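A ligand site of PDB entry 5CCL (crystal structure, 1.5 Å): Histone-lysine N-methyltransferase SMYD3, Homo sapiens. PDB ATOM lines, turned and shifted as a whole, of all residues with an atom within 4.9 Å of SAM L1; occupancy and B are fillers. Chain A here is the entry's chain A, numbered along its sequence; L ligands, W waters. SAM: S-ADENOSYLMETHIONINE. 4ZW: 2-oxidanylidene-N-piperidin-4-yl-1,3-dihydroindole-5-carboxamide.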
ATOM      1  N   ASN A  13      11.860  -4.842 -12.498  1.00  0.00           N
ATOM      2  CA  ASN A  13      12.250  -5.599 -11.321  1.00  0.00           C
ATOM      3  C   ASN A  13      11.357  -6.753 -10.977  1.00  0.00           C
ATOM      4  O   ASN A  13      11.461  -7.309  -9.884  1.00  0.00           O
ATOM      5  CB  ASN A  13      12.425  -4.708 -10.082  1.00  0.00           C
ATOM      6  CG  ASN A  13      11.185  -3.937  -9.731  1.00  0.00           C
ATOM      7  OD1 ASN A  13      10.096  -4.486  -9.707  1.00  0.00           O
ATOM      8  ND2 ASN A  13      11.347  -2.690  -9.420  1.00  0.00           N
ATOM      9  N   ARG A  14      10.519  -7.175 -11.902  1.00  0.00           N
ATOM     10  CA  ARG A  14       9.681  -8.364 -11.602  1.00  0.00           C
ATOM     11  C   ARG A  14       9.637  -9.315 -12.802  1.00  0.00           C
ATOM     12  O   ARG A  14       8.613  -9.938 -13.080  1.00  0.00           O
ATOM     13  CB  ARG A  14       8.299  -8.010 -11.063  1.00  0.00           C
ATOM     14  CG  ARG A  14       7.506  -7.012 -11.848  1.00  0.00           C
ATOM     15  CD  ARG A  14       6.437  -6.296 -10.989  1.00  0.00           C
ATOM     16  NE  ARG A  14       7.189  -5.510 -10.051  1.00  0.00           N
ATOM     17  CZ  ARG A  14       6.736  -4.901  -8.973  1.00  0.00           C
ATOM     18  NH1 ARG A  14       5.450  -4.934  -8.633  1.00  0.00           N
ATOM     19  NH2 ARG A  14       7.636  -4.276  -8.215  1.00  0.00           N
ATOM     20  N   GLY A  15      10.759  -9.449 -13.503  1.00  0.00           N
ATOM     21  CA  GLY A  15      10.801 -10.408 -14.568  1.00  0.00           C
ATOM     22  C   GLY A  15      10.053  -9.940 -15.792  1.00  0.00           C
ATOM     23  O   GLY A  15       9.956  -8.748 -16.092  1.00  0.00           O
ATOM     24  N   ASN A  16       9.519 -10.894 -16.522  1.00  0.00           N
ATOM     25  CA  ASN A  16       8.652 -10.560 -17.621  1.00  0.00           C
ATOM     26  C   ASN A  16       7.265 -10.232 -17.107  1.00  0.00           C
ATOM     27  O   ASN A  16       6.865 -10.655 -16.020  1.00  0.00           O
ATOM     28  CB  ASN A  16       8.600 -11.695 -18.639  1.00  0.00           C
ATOM     29  CG  ASN A  16       9.971 -12.006 -19.233  1.00  0.00           C
ATOM     30  OD1 ASN A  16      10.426 -13.183 -19.276  1.00  0.00           O
ATOM     31  ND2 ASN A  16      10.648 -10.982 -19.609  1.00  0.00           N
ATOM     32  N   TYR A 124       3.934 -17.075 -24.375  1.00  0.00           N
ATOM     33  CA  TYR A 124       4.939 -17.505 -23.406  1.00  0.00           C
ATOM     34  C   TYR A 124       4.776 -19.030 -23.295  1.00  0.00           C
ATOM     35  O   TYR A 124       3.654 -19.531 -23.214  1.00  0.00           O
ATOM     36  CB  TYR A 124       4.666 -16.871 -22.061  1.00  0.00           C
ATOM     37  CG  TYR A 124       5.804 -16.590 -21.111  1.00  0.00           C
ATOM     38  CD1 TYR A 124       6.963 -15.934 -21.531  1.00  0.00           C
ATOM     39  CD2 TYR A 124       5.650 -16.854 -19.763  1.00  0.00           C
ATOM     40  CE1 TYR A 124       7.945 -15.563 -20.636  1.00  0.00           C
ATOM     41  CE2 TYR A 124       6.594 -16.464 -18.827  1.00  0.00           C
ATOM     42  CZ  TYR A 124       7.740 -15.824 -19.259  1.00  0.00           C
ATOM     43  OH  TYR A 124       8.692 -15.397 -18.358  1.00  0.00           O
ATOM     44  N   ASP A 128       9.767 -21.005 -21.048  1.00  0.00           N
ATOM     45  CA  ASP A 128       9.984 -19.611 -20.629  1.00  0.00           C
ATOM     46  C   ASP A 128       9.598 -19.352 -19.148  1.00  0.00           C
ATOM     47  O   ASP A 128       9.935 -18.333 -18.590  1.00  0.00           O
ATOM     48  CB  ASP A 128       9.093 -18.651 -21.447  1.00  0.00           C
ATOM     49  CG  ASP A 128       9.422 -18.611 -22.933  1.00  0.00           C
ATOM     50  OD1 ASP A 128      10.623 -18.602 -23.292  1.00  0.00           O
ATOM     51  OD2 ASP A 128       8.458 -18.544 -23.756  1.00  0.00           O
ATOM     52  N   LEU A 129       8.855 -20.262 -18.524  1.00  0.00           N
ATOM     53  CA  LEU A 129       8.276 -19.972 -17.200  1.00  0.00           C
ATOM     54  C   LEU A 129       9.320 -19.735 -16.131  1.00  0.00           C
ATOM     55  O   LEU A 129      10.376 -20.356 -16.143  1.00  0.00           O
ATOM     56  CB  LEU A 129       7.336 -21.086 -16.741  1.00  0.00           C
ATOM     57  CG  LEU A 129       6.091 -21.333 -17.599  1.00  0.00           C
ATOM     58  CD1 LEU A 129       5.391 -22.574 -17.077  1.00  0.00           C
ATOM     59  CD2 LEU A 129       5.198 -20.108 -17.552  1.00  0.00           C
ATOM     60  N   GLU A 130       8.976 -18.830 -15.213  1.00  0.00           N
ATOM     61  CA  GLU A 130       9.837 -18.536 -14.104  1.00  0.00           C
ATOM     62  C   GLU A 130       9.933 -19.712 -13.173  1.00  0.00           C
ATOM     63  O   GLU A 130       8.902 -20.287 -12.824  1.00  0.00           O
ATOM     64  CB  GLU A 130       9.256 -17.343 -13.356  1.00  0.00           C
ATOM     65  CG  GLU A 130      10.016 -16.971 -12.118  1.00  0.00           C
ATOM     66  CD  GLU A 130      11.413 -16.448 -12.434  1.00  0.00           C
ATOM     67  OE1 GLU A 130      11.510 -15.278 -12.991  1.00  0.00           O
ATOM     68  OE2 GLU A 130      12.436 -17.147 -12.136  1.00  0.00           O
ATOM     69  N   ASN A 132      12.300 -19.278 -10.255  1.00  0.00           N
ATOM     70  CA  ASN A 132      12.795 -18.693  -9.018  1.00  0.00           C
ATOM     71  C   ASN A 132      13.872 -19.545  -8.366  1.00  0.00           C
ATOM     72  O   ASN A 132      14.008 -19.523  -7.128  1.00  0.00           O
ATOM     73  CB  ASN A 132      11.675 -18.451  -7.985  1.00  0.00           C
ATOM     74  CG  ASN A 132      10.592 -17.488  -8.437  1.00  0.00           C
ATOM     75  OD1 ASN A 132       9.424 -17.864  -8.439  1.00  0.00           O
ATOM     76  ND2 ASN A 132      10.956 -16.342  -8.831  1.00  0.00           N
ATOM     77  N   CYS A 180       5.153 -22.176  -9.022  1.00  0.00           N
ATOM     78  CA  CYS A 180       4.781 -20.787  -9.103  1.00  0.00           C
ATOM     79  C   CYS A 180       3.995 -20.415 -10.324  1.00  0.00           C
ATOM     80  O   CYS A 180       3.775 -19.208 -10.526  1.00  0.00           O
ATOM     81  CB  CYS A 180       5.968 -19.846  -8.927  1.00  0.00           C
ATOM     82  SG  CYS A 180       7.191 -20.110 -10.181  1.00  0.00           S
ATOM     83  N   ASN A 181       3.616 -21.421 -11.155  1.00  0.00           N
ATOM     84  CA  ASN A 181       2.802 -21.143 -12.342  1.00  0.00           C
ATOM     85  C   ASN A 181       1.548 -22.005 -12.488  1.00  0.00           C
ATOM     86  O   ASN A 181       0.901 -21.952 -13.499  1.00  0.00           O
ATOM     87  CB  ASN A 181       3.670 -21.293 -13.587  1.00  0.00           C
ATOM     88  CG  ASN A 181       4.778 -20.257 -13.643  1.00  0.00           C
ATOM     89  OD1 ASN A 181       4.568 -19.066 -13.940  1.00  0.00           O
ATOM     90  ND2 ASN A 181       5.982 -20.691 -13.343  1.00  0.00           N
ATOM     91  N   SER A 202       0.514 -16.971 -17.394  1.00  0.00           N
ATOM     92  CA  SER A 202       1.562 -16.835 -16.402  1.00  0.00           C
ATOM     93  C   SER A 202       2.449 -15.641 -16.608  1.00  0.00           C
ATOM     94  O   SER A 202       3.243 -15.351 -15.706  1.00  0.00           O
ATOM     95  CB  SER A 202       2.386 -18.091 -16.316  1.00  0.00           C
ATOM     96  OG  SER A 202       1.653 -19.177 -15.760  1.00  0.00           O
ATOM     97  N   LEU A 203       2.320 -14.893 -17.711  1.00  0.00           N
ATOM     98  CA  LEU A 203       3.038 -13.668 -17.860  1.00  0.00           C
ATOM     99  C   LEU A 203       2.579 -12.607 -16.893  1.00  0.00           C
ATOM    100  O   LEU A 203       3.368 -11.712 -16.574  1.00  0.00           O
ATOM    101  CB  LEU A 203       2.919 -13.072 -19.292  1.00  0.00           C
ATOM    102  CG  LEU A 203       3.947 -13.582 -20.231  1.00  0.00           C
ATOM    103  CD1 LEU A 203       3.554 -13.089 -21.614  1.00  0.00           C
ATOM    104  CD2 LEU A 203       5.354 -13.125 -19.807  1.00  0.00           C
ATOM    105  N   LEU A 204       1.336 -12.667 -16.433  1.00  0.00           N
ATOM    106  CA  LEU A 204       0.787 -11.619 -15.594  1.00  0.00           C
ATOM    107  C   LEU A 204       1.404 -11.617 -14.211  1.00  0.00           C
ATOM    108  O   LEU A 204       1.324 -12.611 -13.493  1.00  0.00           O
ATOM    109  CB  LEU A 204      -0.724 -11.795 -15.441  1.00  0.00           C
ATOM    110  CG  LEU A 204      -1.520 -11.594 -16.740  1.00  0.00           C
ATOM    111  CD1 LEU A 204      -2.741 -12.481 -16.777  1.00  0.00           C
ATOM    112  CD2 LEU A 204      -1.920 -10.143 -16.853  1.00  0.00           C
ATOM    113  N   ASN A 205       1.968 -10.490 -13.806  1.00  0.00           N
ATOM    114  CA  ASN A 205       2.392 -10.324 -12.447  1.00  0.00           C
ATOM    115  C   ASN A 205       1.187 -10.061 -11.507  1.00  0.00           C
ATOM    116  O   ASN A 205       0.066  -9.798 -11.922  1.00  0.00           O
ATOM    117  CB  ASN A 205       3.462  -9.261 -12.380  1.00  0.00           C
ATOM    118  CG  ASN A 205       4.777  -9.768 -12.978  1.00  0.00           C
ATOM    119  OD1 ASN A 205       5.218 -10.854 -12.632  1.00  0.00           O
ATOM    120  ND2 ASN A 205       5.356  -9.010 -13.859  1.00  0.00           N
ATOM    121  N   HIS A 206       1.493 -10.153 -10.207  1.00  0.00           N
ATOM    122  CA  HIS A 206       0.495 -10.073  -9.143  1.00  0.00           C
ATOM    123  C   HIS A 206       0.299  -8.648  -8.650  1.00  0.00           C
ATOM    124  O   HIS A 206       1.289  -7.893  -8.505  1.00  0.00           O
ATOM    125  CB  HIS A 206       0.961 -10.915  -7.965  1.00  0.00           C
ATOM    126  CG  HIS A 206       0.219 -10.688  -6.701  1.00  0.00           C
ATOM    127  ND1 HIS A 206      -0.995 -11.278  -6.426  1.00  0.00           N
ATOM    128  CD2 HIS A 206       0.482  -9.840  -5.667  1.00  0.00           C
ATOM    129  CE1 HIS A 206      -1.428 -10.820  -5.270  1.00  0.00           C
ATOM    130  NE2 HIS A 206      -0.565  -9.944  -4.798  1.00  0.00           N
ATOM    131  N   TYR A 239      -3.114 -13.122  -7.326  1.00  0.00           N
ATOM    132  CA  TYR A 239      -2.823 -14.557  -7.196  1.00  0.00           C
ATOM    133  C   TYR A 239      -3.566 -15.234  -6.067  1.00  0.00           C
ATOM    134  O   TYR A 239      -3.579 -16.445  -5.959  1.00  0.00           O
ATOM    135  CB  TYR A 239      -1.308 -14.817  -7.033  1.00  0.00           C
ATOM    136  CG  TYR A 239      -0.397 -14.445  -8.182  1.00  0.00           C
ATOM    137  CD1 TYR A 239      -0.832 -13.870  -9.340  1.00  0.00           C
ATOM    138  CD2 TYR A 239       0.945 -14.648  -8.050  1.00  0.00           C
ATOM    139  CE1 TYR A 239       0.065 -13.557 -10.367  1.00  0.00           C
ATOM    140  CE2 TYR A 239       1.843 -14.324  -9.024  1.00  0.00           C
ATOM    141  CZ  TYR A 239       1.404 -13.775 -10.207  1.00  0.00           C
ATOM    142  OH  TYR A 239       2.339 -13.471 -11.162  1.00  0.00           O
ATOM    143  N   TYR A 257       5.673 -18.010  -4.286  1.00  0.00           N
ATOM    144  CA  TYR A 257       6.061 -17.162  -5.437  1.00  0.00           C
ATOM    145  C   TYR A 257       7.381 -16.440  -5.268  1.00  0.00           C
ATOM    146  O   TYR A 257       7.833 -15.763  -6.149  1.00  0.00           O
ATOM    147  CB  TYR A 257       4.952 -16.163  -5.772  1.00  0.00           C
ATOM    148  CG  TYR A 257       3.670 -16.823  -6.162  1.00  0.00           C
ATOM    149  CD1 TYR A 257       3.545 -17.344  -7.439  1.00  0.00           C
ATOM    150  CD2 TYR A 257       2.614 -16.969  -5.279  1.00  0.00           C
ATOM    151  CE1 TYR A 257       2.387 -17.934  -7.831  1.00  0.00           C
ATOM    152  CE2 TYR A 257       1.450 -17.597  -5.677  1.00  0.00           C
ATOM    153  CZ  TYR A 257       1.345 -18.061  -6.955  1.00  0.00           C
ATOM    154  OH  TYR A 257       0.171 -18.692  -7.384  1.00  0.00           O
ATOM    155  N   CYS A 258       8.026 -16.591  -4.101  1.00  0.00           N
ATOM    156  CA  CYS A 258       9.334 -15.978  -3.880  1.00  0.00           C
ATOM    157  C   CYS A 258       9.403 -14.498  -4.237  1.00  0.00           C
ATOM    158  O   CYS A 258      10.378 -14.035  -4.839  1.00  0.00           O
ATOM    159  CB  CYS A 258      10.448 -16.711  -4.627  1.00  0.00           C
ATOM    160  SG  CYS A 258      10.680 -18.417  -4.119  1.00  0.00           S
ATOM    161  N   PHE A 259       8.444 -13.728  -3.749  1.00  0.00           N
ATOM    162  CA  PHE A 259       8.594 -12.269  -3.820  1.00  0.00           C
ATOM    163  C   PHE A 259       7.946 -11.545  -2.674  1.00  0.00           C
ATOM    164  O   PHE A 259       7.090 -12.118  -1.971  1.00  0.00           O
ATOM    165  CB  PHE A 259       8.129 -11.665  -5.179  1.00  0.00           C
ATOM    166  CG  PHE A 259       6.646 -11.623  -5.364  1.00  0.00           C
ATOM    167  CD1 PHE A 259       5.949 -12.709  -5.872  1.00  0.00           C
ATOM    168  CD2 PHE A 259       5.943 -10.487  -5.058  1.00  0.00           C
ATOM    169  CE1 PHE A 259       4.587 -12.676  -6.073  1.00  0.00           C
ATOM    170  CE2 PHE A 259       4.556 -10.470  -5.202  1.00  0.00           C
ATOM    171  CZ  PHE A 259       3.880 -11.549  -5.706  1.00  0.00           C
ATOM    172  N   GLU A 260       8.359 -10.282  -2.539  1.00  0.00           N
ATOM    173  CA  GLU A 260       7.863  -9.364  -1.536  1.00  0.00           C
ATOM    174  C   GLU A 260       6.958  -8.357  -2.255  1.00  0.00           C
ATOM    175  O   GLU A 260       7.423  -7.667  -3.163  1.00  0.00           O
ATOM    176  CB  GLU A 260       9.078  -8.645  -0.877  1.00  0.00           C
ATOM    177  CG  GLU A 260      10.294  -9.561  -0.542  1.00  0.00           C
ATOM    178  CD  GLU A 260       9.980 -10.626   0.476  1.00  0.00           C
ATOM    179  OE1 GLU A 260       8.890 -10.501   1.076  1.00  0.00           O
ATOM    180  OE2 GLU A 260      10.820 -11.553   0.728  1.00  0.00           O
ATOM    181  N   CYS A 261       5.668  -8.293  -1.869  1.00  0.00           N
ATOM    182  CA  CYS A 261       4.722  -7.458  -2.618  1.00  0.00           C
ATOM    183  C   CYS A 261       4.882  -5.984  -2.189  1.00  0.00           C
ATOM    184  O   CYS A 261       4.814  -5.642  -0.981  1.00  0.00           O
ATOM    185  CB  CYS A 261       3.282  -7.905  -2.403  1.00  0.00           C
ATOM    186  SG  CYS A 261       2.148  -7.030  -3.491  1.00  0.00           S
HETATM  187  N   SAM L   1       7.412 -12.247 -13.853  1.00  0.00           N
HETATM  188  CA  SAM L   1       7.029 -13.610 -14.276  1.00  0.00           C
HETATM  189  C   SAM L   1       7.965 -14.141 -15.355  1.00  0.00           C
HETATM  190  O   SAM L   1       7.682 -15.246 -15.883  1.00  0.00           O
HETATM  191  OXT SAM L   1       8.974 -13.449 -15.645  1.00  0.00           O
HETATM  192  CB  SAM L   1       5.561 -13.732 -14.669  1.00  0.00           C
HETATM  193  CG  SAM L   1       4.589 -14.047 -13.485  1.00  0.00           C
HETATM  194  SD  SAM L   1       4.868 -15.636 -12.803  1.00  0.00           S
HETATM  195  CE  SAM L   1       3.359 -16.412 -12.696  1.00  0.00           C
HETATM  196  C5' SAM L   1       5.127 -15.386 -11.105  1.00  0.00           C
HETATM  197  C4' SAM L   1       6.484 -14.813 -10.705  1.00  0.00           C
HETATM  198  O4' SAM L   1       6.597 -13.427 -11.095  1.00  0.00           O
HETATM  199  C3' SAM L   1       6.727 -14.781  -9.216  1.00  0.00           C
HETATM  200  O3' SAM L   1       7.134 -16.036  -8.696  1.00  0.00           O
HETATM  201  C2' SAM L   1       7.740 -13.693  -9.117  1.00  0.00           C
HETATM  202  O2' SAM L   1       9.047 -14.114  -9.601  1.00  0.00           O
HETATM  203  C1' SAM L   1       7.226 -12.642 -10.082  1.00  0.00           C
HETATM  204  N9  SAM L   1       6.181 -11.728  -9.566  1.00  0.00           N
HETATM  205  C8  SAM L   1       4.837 -11.771  -9.818  1.00  0.00           C
HETATM  206  N7  SAM L   1       4.242 -10.683  -9.290  1.00  0.00           N
HETATM  207  C5  SAM L   1       5.229  -9.935  -8.680  1.00  0.00           C
HETATM  208  C6  SAM L   1       5.217  -8.695  -7.963  1.00  0.00           C
HETATM  209  N6  SAM L   1       4.085  -8.021  -7.754  1.00  0.00           N
HETATM  210  N1  SAM L   1       6.398  -8.238  -7.480  1.00  0.00           N
HETATM  211  C2  SAM L   1       7.512  -8.957  -7.708  1.00  0.00           C
HETATM  212  N3  SAM L   1       7.632 -10.107  -8.404  1.00  0.00           N
HETATM  213  C4  SAM L   1       6.483 -10.609  -8.892  1.00  0.00           C
HETATM  214  O01 4ZW L   2      -4.640 -20.344  -8.613  1.00  0.00           O
HETATM  215  C02 4ZW L   2      -4.326 -19.162  -8.385  1.00  0.00           C
HETATM  216  N03 4ZW L   2      -4.957 -18.531  -7.374  1.00  0.00           N
HETATM  217  C05 4ZW L   2      -5.920 -19.222  -6.473  1.00  0.00           C
HETATM  218  C07 4ZW L   2      -7.283 -19.307  -7.129  1.00  0.00           C
HETATM  219  C10 4ZW L   2      -8.275 -19.921  -6.167  1.00  0.00           C
HETATM  220  N13 4ZW L   2      -8.311 -19.228  -4.880  1.00  0.00           N
HETATM  221  C15 4ZW L   2      -7.017 -19.182  -4.224  1.00  0.00           C
HETATM  222  C18 4ZW L   2      -5.995 -18.510  -5.135  1.00  0.00           C
HETATM  223  C21 4ZW L   2      -3.371 -18.461  -9.275  1.00  0.00           C
HETATM  224  C22 4ZW L   2      -2.343 -19.247  -9.802  1.00  0.00           C
HETATM  225  C24 4ZW L   2      -1.434 -18.685 -10.676  1.00  0.00           C
HETATM  226  C25 4ZW L   2      -1.629 -17.373 -11.094  1.00  0.00           C
HETATM  227  N26 4ZW L   2      -0.629 -17.038 -12.000  1.00  0.00           N
HETATM  228  C28 4ZW L   2       0.197 -18.108 -12.279  1.00  0.00           C
HETATM  229  O29 4ZW L   2       1.087 -18.137 -13.108  1.00  0.00           O
HETATM  230  C30 4ZW L   2      -0.280 -19.251 -11.414  1.00  0.00           C
HETATM  231  C33 4ZW L   2      -2.659 -16.554 -10.633  1.00  0.00           C
HETATM  232  C35 4ZW L   2      -3.553 -17.145  -9.732  1.00  0.00           C
HETATM  233  O   HOH W   1      10.783 -13.574  -7.482  1.00  0.00           O
HETATM  234  O   HOH W   2       9.772 -13.149 -12.337  1.00  0.00           O
HETATM  235  O   HOH W   3       6.410 -17.669 -15.440  1.00  0.00           O
HETATM  236  O   HOH W   4       3.485  -5.700  -6.054  1.00  0.00           O
HETATM  237  O   HOH W   5      10.343 -10.890  -8.311  1.00  0.00           O
HETATM  238  O   HOH W   6      11.387 -14.617 -15.823  1.00  0.00           O
HETATM  239  O   HOH W   7       6.756  -6.302  -5.445  1.00  0.00           O
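An oxygen (OXT) of SAM L1 sits at hydrogen-bond distance from the backbone NH (N) of Asn 16.
A nitrogen (N) of SAM L1 sits at hydrogen-bond distance from the backbone carbonyl oxygen of Arg 14.
N of His 206 sits at hydrogen-bond distance from N7 of SAM L1 (2.9 Å).
An oxygen (O3') of SAM L1 is in hydrogen-bond range of the backbone carbonyl oxygen (O) of Tyr 257 (2.7 Å).
A nitrogen (N03) of 4ZW L2 lies within hydrogen-bond range of the backbone carbonyl oxygen (O) of Tyr 239 (2.9 Å).
A nitrogen (N6) of SAM L1 lies within hydrogen-bond range of the backbone carbonyl oxygen of His 206 (2.9 Å).
OD1 of Asn 132 is in hydrogen-bond range of O3' of SAM L1.
O29 of 4ZW L2 sits at hydrogen-bond distance from OG of Ser 202.
The side-chain amide oxygen of Asn 205 lies within hydrogen-bond range of a nitrogen (N) of SAM L1 (2.9 Å).
The side-chain hydroxyl (OH) of Tyr 124 is in hydrogen-bond range of an oxygen (O) of SAM L1.
O of Asn 16 sits at hydrogen-bond distance from N of SAM L1 (2.7 Å).
The backbone carbonyl oxygen (O) of Arg 14 sits at hydrogen-bond distance from the side-chain amide nitrogen (ND2) of Asn 205, 3.5 Å away.
The side-chain sulfur of Cys 180 lies within hydrogen-bond range of the backbone carbonyl oxygen of Glu 130.
The side-chain amide oxygen (OD1) of Asn 132 is in hydrogen-bond range of the side-chain sulfur (SG) of Cys 180 (3.6 Å).
SG of Cys 180 lies within hydrogen-bond range of ND2 of Asn 181 (3.4 Å).
The side-chain carboxylate (OE2) of Glu 130 is in hydrogen-bond range of the backbone NH (N) of Asn 132 (2.8 Å).
The side-chain amide nitrogen (ND2) of Asn 181 is in hydrogen-bond range of the backbone carbonyl oxygen (O) of Glu 130 (3.0 Å).
The guanidinium group (NH2) of Arg 14 lies within hydrogen-bond range of the side-chain amide oxygen (OD1) of Asn 13, at 2.9 Å.
The side-chain hydroxyl (OG) of Ser 202 lies close to the side-chain amide oxygen (OD1) of Asn 181, at 3.4 Å.
The side-chain amide oxygen (OD1) of Asn 181 lies close to a sulfur (SD) of SAM L1, at 3.6 Å.
The backbone carbonyl oxygen (O) of Ser 202 sits close to a sulfur (SD) of SAM L1.
SD of SAM L1 lies close to OH of Tyr 239 (3.7 Å).
Gly 15 touches SAM L1 (C to OXT, 3.7 Å).
CB of Glu 130 touches O of SAM L1, at 3.6 Å.
O of Cys 180 touches CE of SAM L1 (3.6 Å).
Leu 203 touches SAM L1 (O to CB, 3.5 Å).
Leu 204 touches SAM L1.
Phe 259 touches SAM L1.
16 residues have an atom within 4 Å of SAM L1: Arg 14, Gly 15, Asn 16, Tyr 124, Glu 130, Asn 132, Cys 180, Asn 181, Ser 202, Leu 203, Leu 204, Asn 205, His 206, Tyr 239, Tyr 257 and Phe 259.
Along chain A the residues within 4 Å of SAM L1 span positions 14 to 259.
The nearest printed residue that does not touch SAM L1 is Glu 260 (4.5 Å).
Water W6 bridges an oxygen (OXT) of SAM L1 (2.7 Å) and the side-chain carboxylate of Glu 130 (2.9 Å).
Water W3 lies within hydrogen-bond range of the side-chain amide oxygen of Asn 181, an oxygen (O) of SAM L1 and the backbone NH of Glu 130.
Water W1 lies within hydrogen-bond range of O of Cys 258, O2' of SAM L1 and ND2 of Asn 132.
Water W7 lies within hydrogen-bond range of O of Glu 260 (2.7 Å) and N1 of SAM L1 (2.8 Å).
Water W4 lies within hydrogen-bond range of N6 of SAM L1 and NH1 of Arg 14.
Water W2 lies within hydrogen-bond range of OE1 of Glu 130 (2.8 Å), N of SAM L1 (2.9 Å) and O of Arg 14 (3.5 Å).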
